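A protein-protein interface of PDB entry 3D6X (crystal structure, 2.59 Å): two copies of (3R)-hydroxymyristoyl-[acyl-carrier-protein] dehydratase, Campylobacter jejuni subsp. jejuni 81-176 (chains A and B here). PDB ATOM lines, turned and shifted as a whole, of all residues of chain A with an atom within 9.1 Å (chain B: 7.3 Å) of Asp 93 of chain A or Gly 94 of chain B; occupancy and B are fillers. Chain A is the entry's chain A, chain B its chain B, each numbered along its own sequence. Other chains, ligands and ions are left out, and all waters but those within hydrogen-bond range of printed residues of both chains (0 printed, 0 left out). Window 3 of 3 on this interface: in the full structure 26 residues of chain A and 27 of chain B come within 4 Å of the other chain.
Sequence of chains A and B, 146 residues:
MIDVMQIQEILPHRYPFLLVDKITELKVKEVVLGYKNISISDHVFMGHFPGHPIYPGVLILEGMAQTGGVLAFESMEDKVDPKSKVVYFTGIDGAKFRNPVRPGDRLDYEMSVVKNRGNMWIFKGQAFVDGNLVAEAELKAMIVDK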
ATOM      1  N   LEU A  61     -15.294 -11.695  19.453  1.00  0.00           N
ATOM      2  CA  LEU A  61     -13.879 -11.830  19.794  1.00  0.00           C
ATOM      3  C   LEU A  61     -13.684 -12.667  21.061  1.00  0.00           C
ATOM      4  O   LEU A  61     -12.774 -13.482  21.121  1.00  0.00           O
ATOM      5  CB  LEU A  61     -13.220 -10.468  20.005  1.00  0.00           C
ATOM      6  CG  LEU A  61     -13.209  -9.402  18.901  1.00  0.00           C
ATOM      7  CD1 LEU A  61     -12.811  -8.025  19.463  1.00  0.00           C
ATOM      8  CD2 LEU A  61     -12.314  -9.785  17.748  1.00  0.00           C
ATOM      9  N   MET A  64     -14.077 -16.316  20.187  1.00  0.00           N
ATOM     10  CA  MET A  64     -12.858 -16.769  19.566  1.00  0.00           C
ATOM     11  C   MET A  64     -11.830 -17.047  20.643  1.00  0.00           C
ATOM     12  O   MET A  64     -11.235 -18.125  20.687  1.00  0.00           O
ATOM     13  CB  MET A  64     -12.316 -15.739  18.589  1.00  0.00           C
ATOM     14  CG  MET A  64     -13.193 -15.575  17.352  1.00  0.00           C
ATOM     15  SD  MET A  64     -12.473 -14.267  16.050  1.00  0.00           S
ATOM     16  CE  MET A  64     -11.321 -13.243  17.245  1.00  0.00           C
ATOM     17  N   PHE A  89      -5.269 -13.582  27.603  1.00  0.00           N
ATOM     18  CA  PHE A  89      -5.169 -12.919  26.299  1.00  0.00           C
ATOM     19  C   PHE A  89      -4.755 -11.473  26.459  1.00  0.00           C
ATOM     20  O   PHE A  89      -5.502 -10.672  26.989  1.00  0.00           O
ATOM     21  CB  PHE A  89      -6.483 -13.036  25.548  1.00  0.00           C
ATOM     22  CG  PHE A  89      -6.606 -14.324  24.799  1.00  0.00           C
ATOM     23  CD1 PHE A  89      -6.355 -14.382  23.445  1.00  0.00           C
ATOM     24  CD2 PHE A  89      -6.899 -15.496  25.458  1.00  0.00           C
ATOM     25  CE1 PHE A  89      -6.439 -15.565  22.764  1.00  0.00           C
ATOM     26  CE2 PHE A  89      -6.971 -16.707  24.764  1.00  0.00           C
ATOM     27  CZ  PHE A  89      -6.749 -16.726  23.415  1.00  0.00           C
ATOM     28  N   THR A  90      -3.564 -11.127  26.015  1.00  0.00           N
ATOM     29  CA  THR A  90      -3.082  -9.799  26.294  1.00  0.00           C
ATOM     30  C   THR A  90      -3.210  -8.842  25.123  1.00  0.00           C
ATOM     31  O   THR A  90      -2.975  -7.635  25.286  1.00  0.00           O
ATOM     32  CB  THR A  90      -1.640  -9.822  26.777  1.00  0.00           C
ATOM     33  OG1 THR A  90      -0.833 -10.518  25.829  1.00  0.00           O
ATOM     34  CG2 THR A  90      -1.565 -10.527  28.097  1.00  0.00           C
ATOM     35  N   GLY A  91      -3.568  -9.368  23.953  1.00  0.00           N
ATOM     36  CA  GLY A  91      -3.632  -8.545  22.748  1.00  0.00           C
ATOM     37  C   GLY A  91      -4.561  -9.006  21.645  1.00  0.00           C
ATOM     38  O   GLY A  91      -4.753 -10.200  21.416  1.00  0.00           O
ATOM     39  N   ILE A  92      -5.167  -8.041  20.967  1.00  0.00           N
ATOM     40  CA  ILE A  92      -5.957  -8.318  19.780  1.00  0.00           C
ATOM     41  C   ILE A  92      -5.574  -7.306  18.732  1.00  0.00           C
ATOM     42  O   ILE A  92      -5.413  -6.115  19.029  1.00  0.00           O
ATOM     43  CB  ILE A  92      -7.480  -8.201  20.014  1.00  0.00           C
ATOM     44  CG1 ILE A  92      -7.948  -9.142  21.119  1.00  0.00           C
ATOM     45  CG2 ILE A  92      -8.247  -8.512  18.725  1.00  0.00           C
ATOM     46  CD1 ILE A  92      -9.363  -8.885  21.557  1.00  0.00           C
ATOM     47  N   ASP A  93      -5.432  -7.780  17.500  1.00  0.00           N
ATOM     48  CA  ASP A  93      -4.982  -6.933  16.422  1.00  0.00           C
ATOM     49  C   ASP A  93      -5.661  -7.205  15.083  1.00  0.00           C
ATOM     50  O   ASP A  93      -6.089  -8.314  14.800  1.00  0.00           O
ATOM     51  CB  ASP A  93      -3.490  -7.047  16.292  1.00  0.00           C
ATOM     52  CG  ASP A  93      -2.895  -5.800  15.764  1.00  0.00           C
ATOM     53  OD1 ASP A  93      -1.664  -5.776  15.521  1.00  0.00           O
ATOM     54  OD2 ASP A  93      -3.672  -4.836  15.588  1.00  0.00           O
ATOM     55  N   GLY A  94      -5.760  -6.178  14.257  1.00  0.00           N
ATOM     56  CA  GLY A  94      -6.446  -6.297  12.986  1.00  0.00           C
ATOM     57  C   GLY A  94      -7.831  -6.901  13.107  1.00  0.00           C
ATOM     58  O   GLY A  94      -8.219  -7.742  12.300  1.00  0.00           O
ATOM     59  N   ALA A  95      -8.578  -6.496  14.127  1.00  0.00           N
ATOM     60  CA  ALA A  95      -9.930  -7.007  14.305  1.00  0.00           C
ATOM     61  C   ALA A  95     -10.849  -6.263  13.376  1.00  0.00           C
ATOM     62  O   ALA A  95     -10.827  -5.038  13.314  1.00  0.00           O
ATOM     63  CB  ALA A  95     -10.404  -6.834  15.726  1.00  0.00           C
ATOM     64  N   LYS A  96     -11.663  -7.007  12.649  1.00  0.00           N
ATOM     65  CA  LYS A  96     -12.568  -6.415  11.696  1.00  0.00           C
ATOM     66  C   LYS A  96     -13.914  -7.081  11.867  1.00  0.00           C
ATOM     67  O   LYS A  96     -13.976  -8.295  12.041  1.00  0.00           O
ATOM     68  CB  LYS A  96     -12.057  -6.630  10.282  1.00  0.00           C
ATOM     69  CG  LYS A  96     -10.800  -5.843   9.922  1.00  0.00           C
ATOM     70  CD  LYS A  96     -10.120  -6.504   8.760  1.00  0.00           C
ATOM     71  CE  LYS A  96      -9.314  -5.519   7.926  1.00  0.00           C
ATOM     72  NZ  LYS A  96      -8.009  -5.188   8.541  1.00  0.00           N
ATOM     73  N   ILE A 122      -0.002 -17.054  19.315  1.00  0.00           N
ATOM     74  CA  ILE A 122      -0.622 -16.070  18.455  1.00  0.00           C
ATOM     75  C   ILE A 122      -1.563 -16.794  17.515  1.00  0.00           C
ATOM     76  O   ILE A 122      -1.171 -17.728  16.834  1.00  0.00           O
ATOM     77  CB  ILE A 122       0.435 -15.270  17.673  1.00  0.00           C
ATOM     78  CG1 ILE A 122       1.449 -14.649  18.637  1.00  0.00           C
ATOM     79  CG2 ILE A 122      -0.220 -14.211  16.819  1.00  0.00           C
ATOM     80  CD1 ILE A 122       2.323 -13.642  17.989  1.00  0.00           C
ATOM     81  N   PHE A 123      -2.817 -16.374  17.500  1.00  0.00           N
ATOM     82  CA  PHE A 123      -3.810 -17.039  16.693  1.00  0.00           C
ATOM     83  C   PHE A 123      -4.361 -16.145  15.620  1.00  0.00           C
ATOM     84  O   PHE A 123      -4.556 -14.948  15.833  1.00  0.00           O
ATOM     85  CB  PHE A 123      -5.009 -17.449  17.516  1.00  0.00           C
ATOM     86  CG  PHE A 123      -4.680 -18.185  18.755  1.00  0.00           C
ATOM     87  CD1 PHE A 123      -4.298 -17.500  19.906  1.00  0.00           C
ATOM     88  CD2 PHE A 123      -4.802 -19.552  18.803  1.00  0.00           C
ATOM     89  CE1 PHE A 123      -4.021 -18.171  21.079  1.00  0.00           C
ATOM     90  CE2 PHE A 123      -4.517 -20.228  19.970  1.00  0.00           C
ATOM     91  CZ  PHE A 123      -4.135 -19.524  21.117  1.00  0.00           C
ATOM     92  N   LYS A 124      -4.652 -16.761  14.481  1.00  0.00           N
ATOM     93  CA  LYS A 124      -5.491 -16.176  13.472  1.00  0.00           C
ATOM     94  C   LYS A 124      -6.905 -16.678  13.792  1.00  0.00           C
ATOM     95  O   LYS A 124      -7.142 -17.879  13.881  1.00  0.00           O
ATOM     96  CB  LYS A 124      -5.056 -16.685  12.108  1.00  0.00           C
ATOM     97  CG  LYS A 124      -5.399 -15.801  10.921  1.00  0.00           C
ATOM     98  CD  LYS A 124      -5.831 -16.663   9.727  1.00  0.00           C
ATOM     99  CE  LYS A 124      -5.696 -15.946   8.389  1.00  0.00           C
ATOM    100  NZ  LYS A 124      -4.431 -16.364   7.665  1.00  0.00           N
ATOM    101  N   GLY A 125      -7.838 -15.756  13.985  1.00  0.00           N
ATOM    102  CA  GLY A 125      -9.201 -16.120  14.306  1.00  0.00           C
ATOM    103  C   GLY A 125     -10.191 -15.546  13.313  1.00  0.00           C
ATOM    104  O   GLY A 125     -10.041 -14.404  12.833  1.00  0.00           O
ATOM    105  N   GLU A 136     -12.946 -11.105  12.217  1.00  0.00           N
ATOM    106  CA  GLU A 136     -11.623 -11.710  12.198  1.00  0.00           C
ATOM    107  C   GLU A 136     -10.647 -10.880  12.996  1.00  0.00           C
ATOM    108  O   GLU A 136     -10.840  -9.680  13.160  1.00  0.00           O
ATOM    109  CB  GLU A 136     -11.138 -11.854  10.773  1.00  0.00           C
ATOM    110  CG  GLU A 136     -11.028 -10.540  10.057  1.00  0.00           C
ATOM    111  CD  GLU A 136     -10.576 -10.733   8.646  1.00  0.00           C
ATOM    112  OE1 GLU A 136     -11.255 -10.225   7.726  1.00  0.00           O
ATOM    113  OE2 GLU A 136      -9.548 -11.417   8.456  1.00  0.00           O
ATOM    114  N   ALA A 137      -9.602 -11.527  13.490  1.00  0.00           N
ATOM    115  CA  ALA A 137      -8.619 -10.839  14.298  1.00  0.00           C
ATOM    116  C   ALA A 137      -7.439 -11.753  14.589  1.00  0.00           C
ATOM    117  O   ALA A 137      -7.526 -12.965  14.411  1.00  0.00           O
ATOM    118  CB  ALA A 137      -9.262 -10.358  15.590  1.00  0.00           C
ATOM    119  N   GLU A 138      -6.336 -11.159  15.026  1.00  0.00           N
ATOM    120  CA  GLU A 138      -5.196 -11.917  15.482  1.00  0.00           C
ATOM    121  C   GLU A 138      -5.150 -11.772  16.976  1.00  0.00           C
ATOM    122  O   GLU A 138      -5.135 -10.657  17.487  1.00  0.00           O
ATOM    123  CB  GLU A 138      -3.923 -11.338  14.886  1.00  0.00           C
ATOM    124  CG  GLU A 138      -3.019 -12.378  14.261  1.00  0.00           C
ATOM    125  CD  GLU A 138      -1.645 -11.855  14.014  1.00  0.00           C
ATOM    126  OE1 GLU A 138      -1.106 -12.142  12.932  1.00  0.00           O
ATOM    127  OE2 GLU A 138      -1.106 -11.146  14.891  1.00  0.00           O
ATOM    128  N   LEU A 139      -5.152 -12.883  17.701  1.00  0.00           N
ATOM    129  CA  LEU A 139      -5.168 -12.789  19.166  1.00  0.00           C
ATOM    130  C   LEU A 139      -3.860 -13.274  19.749  1.00  0.00           C
ATOM    131  O   LEU A 139      -3.315 -14.309  19.333  1.00  0.00           O
ATOM    132  CB  LEU A 139      -6.323 -13.571  19.784  1.00  0.00           C
ATOM    133  CG  LEU A 139      -7.668 -13.690  19.064  1.00  0.00           C
ATOM    134  CD1 LEU A 139      -8.758 -14.064  20.046  1.00  0.00           C
ATOM    135  CD2 LEU A 139      -8.064 -12.413  18.398  1.00  0.00           C
ATOM    136  N   LYS A 140      -3.344 -12.522  20.708  1.00  0.00           N
ATOM    137  CA  LYS A 140      -2.124 -12.936  21.393  1.00  0.00           C
ATOM    138  C   LYS A 140      -2.464 -13.406  22.808  1.00  0.00           C
ATOM    139  O   LYS A 140      -3.235 -12.751  23.529  1.00  0.00           O
ATOM    140  CB  LYS A 140      -1.102 -11.809  21.425  1.00  0.00           C
ATOM    141  CG  LYS A 140       0.139 -12.144  22.257  1.00  0.00           C
ATOM    142  CD  LYS A 140       0.946 -10.905  22.675  1.00  0.00           C
ATOM    143  CE  LYS A 140       1.974 -10.503  21.637  1.00  0.00           C
ATOM    144  NZ  LYS A 140       3.168  -9.914  22.305  1.00  0.00           N
ATOM    145  N   ILE B  92     -10.748  -2.811  15.167  1.00  0.00           N
ATOM    146  CA  ILE B  92      -9.986  -2.558  16.365  1.00  0.00           C
ATOM    147  C   ILE B  92      -8.576  -3.038  16.133  1.00  0.00           C
ATOM    148  O   ILE B  92      -8.368  -4.104  15.552  1.00  0.00           O
ATOM    149  CB  ILE B  92     -10.576  -3.280  17.533  1.00  0.00           C
ATOM    150  CG1 ILE B  92     -11.942  -2.680  17.872  1.00  0.00           C
ATOM    151  CG2 ILE B  92      -9.646  -3.158  18.708  1.00  0.00           C
ATOM    152  CD1 ILE B  92     -12.761  -3.555  18.680  1.00  0.00           C
ATOM    153  N   ASP B  93      -7.599  -2.233  16.549  1.00  0.00           N
ATOM    154  CA  ASP B  93      -6.182  -2.513  16.274  1.00  0.00           C
ATOM    155  C   ASP B  93      -5.282  -2.243  17.465  1.00  0.00           C
ATOM    156  O   ASP B  93      -5.554  -1.343  18.269  1.00  0.00           O
ATOM    157  CB  ASP B  93      -5.677  -1.663  15.102  1.00  0.00           C
ATOM    158  CG  ASP B  93      -5.815  -2.362  13.785  1.00  0.00           C
ATOM    159  OD1 ASP B  93      -4.944  -2.199  12.899  1.00  0.00           O
ATOM    160  OD2 ASP B  93      -6.810  -3.095  13.651  1.00  0.00           O
ATOM    161  N   GLY B  94      -4.190  -2.999  17.542  1.00  0.00           N
ATOM    162  CA  GLY B  94      -3.214  -2.841  18.605  1.00  0.00           C
ATOM    163  C   GLY B  94      -3.866  -2.735  19.966  1.00  0.00           C
ATOM    164  O   GLY B  94      -3.512  -1.875  20.771  1.00  0.00           O
ATOM    165  N   ALA B  95      -4.829  -3.606  20.236  1.00  0.00           N
ATOM    166  CA  ALA B  95      -5.486  -3.577  21.524  1.00  0.00           C
ATOM    167  C   ALA B  95      -4.655  -4.368  22.505  1.00  0.00           C
ATOM    168  O   ALA B  95      -4.192  -5.467  22.196  1.00  0.00           O
ATOM    169  CB  ALA B  95      -6.895  -4.120  21.428  1.00  0.00           C
ATOM    170  N   LYS B  96      -4.449  -3.793  23.681  1.00  0.00           N
ATOM    171  CA  LYS B  96      -3.568  -4.388  24.658  1.00  0.00           C
ATOM    172  C   LYS B  96      -4.218  -4.332  25.987  1.00  0.00           C
ATOM    173  O   LYS B  96      -4.769  -3.307  26.346  1.00  0.00           O
ATOM    174  CB  LYS B  96      -2.290  -3.589  24.732  1.00  0.00           C
ATOM    175  CG  LYS B  96      -1.502  -3.685  23.466  1.00  0.00           C
ATOM    176  CD  LYS B  96      -0.233  -2.902  23.514  1.00  0.00           C
ATOM    177  CE  LYS B  96       0.703  -3.533  22.522  1.00  0.00           C
ATOM    178  NZ  LYS B  96       0.601  -5.021  22.638  1.00  0.00           N
ATOM    179  N   PHE B  97      -4.145  -5.425  26.734  1.00  0.00           N
ATOM    180  CA  PHE B  97      -4.644  -5.441  28.100  1.00  0.00           C
ATOM    181  C   PHE B  97      -3.503  -5.520  29.074  1.00  0.00           C
ATOM    182  O   PHE B  97      -2.659  -6.388  28.964  1.00  0.00           O
ATOM    183  CB  PHE B  97      -5.606  -6.603  28.305  1.00  0.00           C
ATOM    184  CG  PHE B  97      -6.734  -6.597  27.340  1.00  0.00           C
ATOM    185  CD1 PHE B  97      -6.800  -7.531  26.327  1.00  0.00           C
ATOM    186  CD2 PHE B  97      -7.691  -5.615  27.398  1.00  0.00           C
ATOM    187  CE1 PHE B  97      -7.822  -7.509  25.421  1.00  0.00           C
ATOM    188  CE2 PHE B  97      -8.730  -5.583  26.483  1.00  0.00           C
ATOM    189  CZ  PHE B  97      -8.790  -6.526  25.501  1.00  0.00           C
ATOM    190  N   GLY B 125      -7.779   4.996  21.913  1.00  0.00           N
ATOM    191  CA  GLY B 125      -8.496   4.766  23.156  1.00  0.00           C
ATOM    192  C   GLY B 125      -7.628   4.175  24.252  1.00  0.00           C
ATOM    193  O   GLY B 125      -6.745   3.357  23.995  1.00  0.00           O
ATOM    194  N   ALA B 135      -5.940  -0.751  29.605  1.00  0.00           N
ATOM    195  CA  ALA B 135      -6.116  -1.203  28.245  1.00  0.00           C
ATOM    196  C   ALA B 135      -5.995  -0.066  27.241  1.00  0.00           C
ATOM    197  O   ALA B 135      -6.125   1.106  27.578  1.00  0.00           O
ATOM    198  CB  ALA B 135      -7.432  -1.910  28.101  1.00  0.00           C
ATOM    199  N   GLU B 136      -5.717  -0.426  26.000  1.00  0.00           N
ATOM    200  CA  GLU B 136      -5.612   0.558  24.932  1.00  0.00           C
ATOM    201  C   GLU B 136      -5.875  -0.088  23.577  1.00  0.00           C
ATOM    202  O   GLU B 136      -5.674  -1.304  23.392  1.00  0.00           O
ATOM    203  CB  GLU B 136      -4.243   1.266  24.925  1.00  0.00           C
ATOM    204  CG  GLU B 136      -3.102   0.447  24.388  1.00  0.00           C
ATOM    205  CD  GLU B 136      -1.770   1.208  24.438  1.00  0.00           C
ATOM    206  OE1 GLU B 136      -0.714   0.548  24.656  1.00  0.00           O
ATOM    207  OE2 GLU B 136      -1.760   2.465  24.260  1.00  0.00           O
ATOM    208  N   ALA B 137      -6.302   0.741  22.634  1.00  0.00           N
ATOM    209  CA  ALA B 137      -6.618   0.261  21.314  1.00  0.00           C
ATOM    210  C   ALA B 137      -6.856   1.417  20.375  1.00  0.00           C
ATOM    211  O   ALA B 137      -7.219   2.503  20.821  1.00  0.00           O
ATOM    212  CB  ALA B 137      -7.871  -0.592  21.378  1.00  0.00           C
ATOM    213  N   GLU B 138      -6.676   1.169  19.077  1.00  0.00           N
ATOM    214  CA  GLU B 138      -7.137   2.072  18.048  1.00  0.00           C
ATOM    215  C   GLU B 138      -8.452   1.568  17.491  1.00  0.00           C
ATOM    216  O   GLU B 138      -8.522   0.443  17.032  1.00  0.00           O
ATOM    217  CB  GLU B 138      -6.143   2.081  16.923  1.00  0.00           C
ATOM    218  CG  GLU B 138      -5.259   3.306  16.847  1.00  0.00           C
ATOM    219  CD  GLU B 138      -4.972   3.651  15.418  1.00  0.00           C
ATOM    220  OE1 GLU B 138      -4.004   4.380  15.144  1.00  0.00           O
ATOM    221  OE2 GLU B 138      -5.731   3.169  14.555  1.00  0.00           O
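The backbone NH (N) of Gly 94 of chain B is in hydrogen-bond range of the side-chain carboxylate (OD2) of Asp 93 of chain A (2.7 Å). The side-chain carboxylate (OD2) of Asp 93 of chain B lies close to the backbone NH (N) of Gly 94 of chain A (3.3 Å). N of Ala 95 of chain B lies within hydrogen-bond range of O of Ile 92 of chain A, at 2.8 Å. The backbone carbonyl oxygen of Thr 90 of chain A lies within hydrogen-bond range of the backbone NH of Phe 97 of chain B, at 2.9 Å. O of Ile 92 of chain B lies within hydrogen-bond range of N of Ala 95 of chain A, at 2.8 Å.
The backbone NH of Glu 138 of chain A is in hydrogen-bond range of the backbone carbonyl oxygen of Asp 93 of chain A (2.9 Å). O of Lys 140 of chain A is in hydrogen-bond range of N of Thr 90 of chain A (3.0 Å). N of Lys 140 of chain A sits at hydrogen-bond distance from O of Gly 91 of chain A (2.8 Å). O of Glu 136 of chain B is in hydrogen-bond range of N of Lys 96 of chain B, at 2.8 Å. The backbone carbonyl oxygen (O) of Asp 93 of chain B sits at hydrogen-bond distance from the backbone NH (N) of Glu 138 of chain B, 2.9 Å away.
Phe 97 of chain B touches Phe 89 of chain A. Thr 90 of chain A touches Ala 95 of chain B. O of Thr 90 of chain A touches CA of Lys 96 of chain B, 3.4 Å away. Ala 95 of chain B touches Gly 91 of chain A (O to CA, 3.2 Å). Ile 92 of chain A touches Gly 94 of chain B. Asp 93 of chain A touches Asp 93 of chain B. Gly 94 of chain A touches Ile 92 of chain B (N to O, 3.6 Å). N of Ala 95 of chain A touches OD2 of Asp 93 of chain B, at 3.9 Å.
Of the printed residues of chain B, Asp 93 of chain A touches Asp 93 (3.5 Å) and Gly 94 (2.7 Å). Printed residues of chain A within 4 Å of Ala 95 of chain B: Thr 90, Gly 91 and Ile 92. Printed residues of chain B within 4 Å of Thr 90 of chain A: Ala 95 (3.97 Å), Lys 96 (3.4 Å) and Phe 97 (2.9 Å). Of the printed residues of chain B, Phe 89 of chain A touches Phe 97. Of the printed residues of chain A, Phe 97 of chain B touches Phe 89 and Thr 90. Of the printed residues of chain A, Lys 96 of chain B touches Thr 90 (3.4 Å). Of the printed residues of chain B, Ile 92 of chain A touches Gly 94 (3.7 Å) and Ala 95 (2.8 Å). Phe 123 of chain A touches none of the printed residues of chain B. Gly 125 of chain A touches none of the printed residues of chain B. The nearest printed residue of chain B that does not touch Phe 89 of chain A is Lys 96 of chain B (6.5 Å).
Hydrophobic or aromatic side chains of chain B within 4 Å of the printed part of chain A: Ile 92, Ala 95 and Phe 97. Of the 19 printed residues of chain A, 7 touch a printed residue of chain B. Hydrophobic or aromatic side chains of chain A that line the printed part of chain B: Ala 95. Among the printed residues, no Asp or Glu carboxylate lies within 4 Å of a Lys or Arg side-chain nitrogen of the other chain.
Ile 92 of chain A touches Gly 94 of chain B, and with the chains exchanged Gly 94 of chain A touches Ile 92 of chain B. Ile 92 of chain A touches Ala 95 of chain B, and with the chains exchanged Ala 95 of chain A touches Ile 92 of chain B. Asp 93 of chain A touches Gly 94 of chain B, and with the chains exchanged Gly 94 of chain A touches Asp 93 of chain B. Ala 95 of chain A touches Asp 93 of chain B, but with the chains exchanged Asp 93 of chain A does not touch Ala 95 of chain B (4.9 Å). Of the 13 pairs that touch across the chains among the printed residues, 7 have their exchanged pair printed and touching as well.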
